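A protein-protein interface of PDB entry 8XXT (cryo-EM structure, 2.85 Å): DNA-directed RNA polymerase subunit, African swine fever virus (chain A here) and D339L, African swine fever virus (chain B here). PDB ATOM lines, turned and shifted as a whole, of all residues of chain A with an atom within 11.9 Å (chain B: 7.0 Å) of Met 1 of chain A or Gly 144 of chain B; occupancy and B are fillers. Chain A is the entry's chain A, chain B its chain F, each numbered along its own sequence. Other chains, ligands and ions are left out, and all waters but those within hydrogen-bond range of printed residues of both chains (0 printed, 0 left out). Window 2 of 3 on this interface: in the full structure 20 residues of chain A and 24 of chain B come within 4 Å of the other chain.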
ATOM      1  N   MET A   1      -8.134 -17.905  11.236  1.00  0.00           N
ATOM      2  CA  MET A   1      -8.639 -19.017  10.442  1.00  0.00           C
ATOM      3  C   MET A   1     -10.077 -19.342  10.818  1.00  0.00           C
ATOM      4  O   MET A   1     -10.832 -18.460  11.220  1.00  0.00           O
ATOM      5  CB  MET A   1      -7.749 -20.246  10.616  1.00  0.00           C
ATOM      6  CG  MET A   1      -6.475 -20.182   9.798  1.00  0.00           C
ATOM      7  SD  MET A   1      -5.554 -21.725   9.788  1.00  0.00           S
ATOM      8  CE  MET A   1      -5.458 -22.054  11.539  1.00  0.00           C
ATOM      9  N   GLU A   2     -10.452 -20.611  10.692  1.00  0.00           N
ATOM     10  CA  GLU A   2     -11.816 -21.055  10.937  1.00  0.00           C
ATOM     11  C   GLU A   2     -11.837 -22.047  12.087  1.00  0.00           C
ATOM     12  O   GLU A   2     -11.044 -22.993  12.111  1.00  0.00           O
ATOM     13  CB  GLU A   2     -12.419 -21.693   9.683  1.00  0.00           C
ATOM     14  CG  GLU A   2     -13.860 -22.153   9.838  1.00  0.00           C
ATOM     15  CD  GLU A   2     -14.863 -21.045   9.587  1.00  0.00           C
ATOM     16  OE1 GLU A   2     -14.720 -19.960  10.187  1.00  0.00           O
ATOM     17  OE2 GLU A   2     -15.795 -21.257   8.786  1.00  0.00           O
ATOM     18  N   ALA A   3     -12.741 -21.825  13.033  1.00  0.00           N
ATOM     19  CA  ALA A   3     -13.006 -22.755  14.126  1.00  0.00           C
ATOM     20  C   ALA A   3     -14.373 -23.374  13.866  1.00  0.00           C
ATOM     21  O   ALA A   3     -15.403 -22.750  14.124  1.00  0.00           O
ATOM     22  CB  ALA A   3     -12.957 -22.046  15.473  1.00  0.00           C
ATOM     23  N   GLY A   4     -14.380 -24.598  13.349  1.00  0.00           N
ATOM     24  CA  GLY A   4     -15.629 -25.222  12.970  1.00  0.00           C
ATOM     25  C   GLY A   4     -16.486 -25.583  14.168  1.00  0.00           C
ATOM     26  O   GLY A   4     -15.999 -25.799  15.275  1.00  0.00           O
ATOM     27  N   TYR A   5     -17.790 -25.654  13.924  1.00  0.00           N
ATOM     28  CA  TYR A   5     -18.740 -25.991  14.973  1.00  0.00           C
ATOM     29  C   TYR A   5     -18.432 -27.367  15.547  1.00  0.00           C
ATOM     30  O   TYR A   5     -18.140 -28.314  14.813  1.00  0.00           O
ATOM     31  CB  TYR A   5     -20.160 -25.947  14.412  1.00  0.00           C
ATOM     32  CG  TYR A   5     -21.232 -26.485  15.325  1.00  0.00           C
ATOM     33  CD1 TYR A   5     -21.596 -27.817  15.283  1.00  0.00           C
ATOM     34  CD2 TYR A   5     -21.895 -25.655  16.212  1.00  0.00           C
ATOM     35  CE1 TYR A   5     -22.575 -28.314  16.102  1.00  0.00           C
ATOM     36  CE2 TYR A   5     -22.880 -26.146  17.036  1.00  0.00           C
ATOM     37  CZ  TYR A   5     -23.214 -27.477  16.976  1.00  0.00           C
ATOM     38  OH  TYR A   5     -24.192 -27.983  17.792  1.00  0.00           O
ATOM     39  N   HIS A  64      -9.918 -10.045  23.740  1.00  0.00           N
ATOM     40  CA  HIS A  64     -11.369  -9.963  23.767  1.00  0.00           C
ATOM     41  C   HIS A  64     -11.804  -8.960  24.824  1.00  0.00           C
ATOM     42  O   HIS A  64     -11.140  -8.785  25.849  1.00  0.00           O
ATOM     43  CB  HIS A  64     -12.007 -11.319  24.052  1.00  0.00           C
ATOM     44  CG  HIS A  64     -12.179 -12.174  22.837  1.00  0.00           C
ATOM     45  ND1 HIS A  64     -11.735 -13.477  22.775  1.00  0.00           N
ATOM     46  CD2 HIS A  64     -12.754 -11.916  21.639  1.00  0.00           C
ATOM     47  CE1 HIS A  64     -12.025 -13.982  21.591  1.00  0.00           C
ATOM     48  NE2 HIS A  64     -12.644 -13.056  20.883  1.00  0.00           N
ATOM     49  N   ILE B  34      -9.778 -20.123   3.510  1.00  0.00           N
ATOM     50  CA  ILE B  34      -9.419 -20.341   4.906  1.00  0.00           C
ATOM     51  C   ILE B  34      -7.950 -20.722   5.050  1.00  0.00           C
ATOM     52  O   ILE B  34      -7.243 -20.188   5.912  1.00  0.00           O
ATOM     53  CB  ILE B  34     -10.343 -21.400   5.529  1.00  0.00           C
ATOM     54  CG1 ILE B  34     -11.736 -20.814   5.752  1.00  0.00           C
ATOM     55  CG2 ILE B  34      -9.772 -21.911   6.835  1.00  0.00           C
ATOM     56  CD1 ILE B  34     -12.787 -21.844   6.049  1.00  0.00           C
ATOM     57  N   TYR B  35      -7.458 -21.640   4.219  1.00  0.00           N
ATOM     58  CA  TYR B  35      -6.208 -22.324   4.533  1.00  0.00           C
ATOM     59  C   TYR B  35      -5.029 -21.974   3.637  1.00  0.00           C
ATOM     60  O   TYR B  35      -3.891 -22.241   4.026  1.00  0.00           O
ATOM     61  CB  TYR B  35      -6.417 -23.841   4.501  1.00  0.00           C
ATOM     62  CG  TYR B  35      -7.249 -24.336   5.655  1.00  0.00           C
ATOM     63  CD1 TYR B  35      -6.828 -24.157   6.960  1.00  0.00           C
ATOM     64  CD2 TYR B  35      -8.461 -24.970   5.440  1.00  0.00           C
ATOM     65  CE1 TYR B  35      -7.586 -24.599   8.022  1.00  0.00           C
ATOM     66  CE2 TYR B  35      -9.227 -25.416   6.497  1.00  0.00           C
ATOM     67  CZ  TYR B  35      -8.784 -25.227   7.784  1.00  0.00           C
ATOM     68  OH  TYR B  35      -9.537 -25.668   8.843  1.00  0.00           O
ATOM     69  N   GLY B  37      -2.054 -19.941   2.151  1.00  0.00           N
ATOM     70  CA  GLY B  37      -1.220 -18.877   2.660  1.00  0.00           C
ATOM     71  C   GLY B  37      -0.997 -18.897   4.153  1.00  0.00           C
ATOM     72  O   GLY B  37      -0.347 -17.983   4.674  1.00  0.00           O
ATOM     73  N   LYS B  38      -1.511 -19.900   4.858  1.00  0.00           N
ATOM     74  CA  LYS B  38      -1.368 -20.004   6.302  1.00  0.00           C
ATOM     75  C   LYS B  38      -0.915 -21.407   6.667  1.00  0.00           C
ATOM     76  O   LYS B  38      -1.432 -22.390   6.133  1.00  0.00           O
ATOM     77  CB  LYS B  38      -2.686 -19.683   7.021  1.00  0.00           C
ATOM     78  CG  LYS B  38      -3.179 -18.260   6.826  1.00  0.00           C
ATOM     79  CD  LYS B  38      -4.668 -18.158   7.098  1.00  0.00           C
ATOM     80  CE  LYS B  38      -5.216 -16.809   6.671  1.00  0.00           C
ATOM     81  NZ  LYS B  38      -6.705 -16.785   6.660  1.00  0.00           N
ATOM     82  N   CYS B  39       0.053 -21.496   7.574  1.00  0.00           N
ATOM     83  CA  CYS B  39       0.468 -22.794   8.081  1.00  0.00           C
ATOM     84  C   CYS B  39      -0.597 -23.347   9.016  1.00  0.00           C
ATOM     85  O   CYS B  39      -1.125 -22.629   9.868  1.00  0.00           O
ATOM     86  CB  CYS B  39       1.809 -22.693   8.802  1.00  0.00           C
ATOM     87  SG  CYS B  39       2.096 -21.161   9.687  1.00  0.00           S
ATOM     88  N   PHE B  40      -0.915 -24.626   8.850  1.00  0.00           N
ATOM     89  CA  PHE B  40      -1.992 -25.252   9.605  1.00  0.00           C
ATOM     90  C   PHE B  40      -1.629 -26.708   9.836  1.00  0.00           C
ATOM     91  O   PHE B  40      -1.462 -27.463   8.874  1.00  0.00           O
ATOM     92  CB  PHE B  40      -3.320 -25.127   8.854  1.00  0.00           C
ATOM     93  CG  PHE B  40      -4.414 -26.003   9.394  1.00  0.00           C
ATOM     94  CD1 PHE B  40      -4.964 -25.760  10.638  1.00  0.00           C
ATOM     95  CD2 PHE B  40      -4.899 -27.065   8.649  1.00  0.00           C
ATOM     96  CE1 PHE B  40      -5.971 -26.562  11.130  1.00  0.00           C
ATOM     97  CE2 PHE B  40      -5.906 -27.869   9.136  1.00  0.00           C
ATOM     98  CZ  PHE B  40      -6.441 -27.618  10.376  1.00  0.00           C
ATOM     99  N   LYS B  41      -1.501 -27.094  11.105  1.00  0.00           N
ATOM    100  CA  LYS B  41      -1.190 -28.465  11.502  1.00  0.00           C
ATOM    101  C   LYS B  41       0.167 -28.913  10.953  1.00  0.00           C
ATOM    102  O   LYS B  41       0.276 -29.890  10.212  1.00  0.00           O
ATOM    103  CB  LYS B  41      -2.303 -29.426  11.076  1.00  0.00           C
ATOM    104  CG  LYS B  41      -3.634 -29.158  11.750  1.00  0.00           C
ATOM    105  CD  LYS B  41      -4.425 -30.438  11.975  1.00  0.00           C
ATOM    106  CE  LYS B  41      -4.775 -31.113  10.663  1.00  0.00           C
ATOM    107  NZ  LYS B  41      -5.535 -32.376  10.874  1.00  0.00           N
ATOM    108  N   ILE B  45       0.673 -25.474   3.599  1.00  0.00           N
ATOM    109  CA  ILE B  45      -0.461 -25.417   2.676  1.00  0.00           C
ATOM    110  C   ILE B  45      -0.263 -24.317   1.642  1.00  0.00           C
ATOM    111  O   ILE B  45      -0.604 -23.155   1.882  1.00  0.00           O
ATOM    112  CB  ILE B  45      -1.794 -25.215   3.417  1.00  0.00           C
ATOM    113  CG1 ILE B  45      -1.906 -26.171   4.599  1.00  0.00           C
ATOM    114  CG2 ILE B  45      -2.961 -25.400   2.465  1.00  0.00           C
ATOM    115  CD1 ILE B  45      -3.199 -26.034   5.351  1.00  0.00           C
ATOM    116  N   TYR B 141       6.054 -24.246  12.720  1.00  0.00           N
ATOM    117  CA  TYR B 141       4.871 -23.913  11.932  1.00  0.00           C
ATOM    118  C   TYR B 141       3.730 -23.597  12.893  1.00  0.00           C
ATOM    119  O   TYR B 141       2.833 -24.405  13.128  1.00  0.00           O
ATOM    120  CB  TYR B 141       4.517 -25.058  10.990  1.00  0.00           C
ATOM    121  CG  TYR B 141       5.302 -25.056   9.703  1.00  0.00           C
ATOM    122  CD1 TYR B 141       4.934 -24.236   8.650  1.00  0.00           C
ATOM    123  CD2 TYR B 141       6.411 -25.871   9.540  1.00  0.00           C
ATOM    124  CE1 TYR B 141       5.641 -24.230   7.472  1.00  0.00           C
ATOM    125  CE2 TYR B 141       7.130 -25.869   8.366  1.00  0.00           C
ATOM    126  CZ  TYR B 141       6.740 -25.044   7.335  1.00  0.00           C
ATOM    127  OH  TYR B 141       7.446 -25.031   6.156  1.00  0.00           O
ATOM    128  N   ILE B 142       3.773 -22.393  13.457  1.00  0.00           N
ATOM    129  CA  ILE B 142       2.739 -21.957  14.391  1.00  0.00           C
ATOM    130  C   ILE B 142       1.459 -21.710  13.601  1.00  0.00           C
ATOM    131  O   ILE B 142       1.450 -20.875  12.686  1.00  0.00           O
ATOM    132  CB  ILE B 142       3.175 -20.711  15.175  1.00  0.00           C
ATOM    133  CG1 ILE B 142       3.880 -19.710  14.262  1.00  0.00           C
ATOM    134  CG2 ILE B 142       4.101 -21.103  16.312  1.00  0.00           C
ATOM    135  CD1 ILE B 142       4.302 -18.448  14.971  1.00  0.00           C
ATOM    136  N   PRO B 143       0.366 -22.402  13.924  1.00  0.00           N
ATOM    137  CA  PRO B 143      -0.817 -22.365  13.057  1.00  0.00           C
ATOM    138  C   PRO B 143      -1.393 -20.965  12.920  1.00  0.00           C
ATOM    139  O   PRO B 143      -1.350 -20.153  13.845  1.00  0.00           O
ATOM    140  CB  PRO B 143      -1.801 -23.308  13.759  1.00  0.00           C
ATOM    141  CG  PRO B 143      -1.314 -23.405  15.156  1.00  0.00           C
ATOM    142  CD  PRO B 143       0.166 -23.270  15.092  1.00  0.00           C
ATOM    143  N   GLY B 144      -1.926 -20.689  11.732  1.00  0.00           N
ATOM    144  CA  GLY B 144      -2.530 -19.414  11.428  1.00  0.00           C
ATOM    145  C   GLY B 144      -1.575 -18.352  10.938  1.00  0.00           C
ATOM    146  O   GLY B 144      -2.029 -17.273  10.539  1.00  0.00           O
ATOM    147  N   ARG B 145      -0.274 -18.620  10.944  1.00  0.00           N
ATOM    148  CA  ARG B 145       0.701 -17.620  10.539  1.00  0.00           C
ATOM    149  C   ARG B 145       0.925 -17.662   9.034  1.00  0.00           C
ATOM    150  O   ARG B 145       0.783 -18.703   8.389  1.00  0.00           O
ATOM    151  CB  ARG B 145       2.022 -17.827  11.277  1.00  0.00           C
ATOM    152  CG  ARG B 145       2.262 -16.828  12.400  1.00  0.00           C
ATOM    153  CD  ARG B 145       0.958 -16.413  13.065  1.00  0.00           C
ATOM    154  NE  ARG B 145       1.131 -15.283  13.968  1.00  0.00           N
ATOM    155  CZ  ARG B 145       0.191 -14.384  14.233  1.00  0.00           C
ATOM    156  NH1 ARG B 145      -0.996 -14.434  13.651  1.00  0.00           N
ATOM    157  NH2 ARG B 145       0.450 -13.410  15.099  1.00  0.00           N
ATOM    158  N   GLN B 146       1.271 -16.504   8.476  1.00  0.00           N
ATOM    159  CA  GLN B 146       1.422 -16.378   7.034  1.00  0.00           C
ATOM    160  C   GLN B 146       2.695 -17.026   6.512  1.00  0.00           C
ATOM    161  O   GLN B 146       2.836 -17.172   5.294  1.00  0.00           O
ATOM    162  CB  GLN B 146       1.396 -14.903   6.639  1.00  0.00           C
ATOM    163  CG  GLN B 146       0.601 -14.610   5.384  1.00  0.00           C
ATOM    164  CD  GLN B 146      -0.884 -14.488   5.655  1.00  0.00           C
ATOM    165  OE1 GLN B 146      -1.327 -14.580   6.799  1.00  0.00           O
ATOM    166  NE2 GLN B 146      -1.661 -14.268   4.601  1.00  0.00           N
ATOM    167  N   GLN B 147       3.618 -17.411   7.389  1.00  0.00           N
ATOM    168  CA  GLN B 147       4.884 -17.975   6.949  1.00  0.00           C
ATOM    169  C   GLN B 147       5.476 -18.799   8.081  1.00  0.00           C
ATOM    170  O   GLN B 147       5.114 -18.634   9.248  1.00  0.00           O
ATOM    171  CB  GLN B 147       5.862 -16.881   6.512  1.00  0.00           C
ATOM    172  CG  GLN B 147       6.439 -16.078   7.664  1.00  0.00           C
ATOM    173  CD  GLN B 147       6.018 -14.624   7.630  1.00  0.00           C
ATOM    174  OE1 GLN B 147       6.852 -13.730   7.498  1.00  0.00           O
ATOM    175  NE2 GLN B 147       4.718 -14.380   7.742  1.00  0.00           N
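Met 1 of chain A touches just these residues of chain B: Ile 34 (3.96 Å), Tyr 35 (3.9 Å), Lys 38 (3.8 Å), Phe 40 (3.8 Å) and Gly 144 (3.8 Å). Of the printed residues of chain B, Glu 2 of chain A touches Ile 34. His 64 of chain A touches none of the printed residues of chain B. Of chain A, only Met 1 (3.96 Å) and Glu 2 (3.7 Å) come within 4 Å of Ile 34 of chain B. Of the printed residues of chain A, Tyr 35 of chain B touches Met 1 (3.9 Å). No residue of chain A comes within 4 Å of Cys 39 of chain B. Of the printed residues of chain A, Phe 40 of chain B touches Met 1 (3.8 Å). Ile 45 of chain B touches none of the printed residues of chain A. No residue of chain A comes within 4 Å of Ile 142 of chain B. Gly 144 of chain B touches just one residue of chain A: Met 1 (3.8 Å). No residue of chain A comes within 4 Å of Arg 145 of chain B. No residue of chain A comes within 4 Å of Gln 146 of chain B. The nearest residue of chain A that does not touch Gly 144 of chain B is Glu 2 of chain A (8.0 Å).
The backbone NH (N) of Gly 144 of chain B lies within hydrogen-bond range of the backbone carbonyl oxygen (O) of Cys 39 of chain B, 2.8 Å away.
Of the 6 printed residues of chain A, 2 touch a printed residue of chain B. Hydrophobic or aromatic side chains of chain A that line the printed part of chain B: Met 1. Among the printed residues, 6 pairs touch across the chains.
Among the printed residues, merely in contact across the chains: Glu 2 of chain A with Ile 34 of chain B, Met 1 of chain A with Gly 144 of chain B, Met 1 of chain A with Lys 38 of chain B, Met 1 of chain A with Phe 40 of chain B, Met 1 of chain A with Tyr 35 of chain B and Met 1 of chain A with Ile 34 of chain B.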
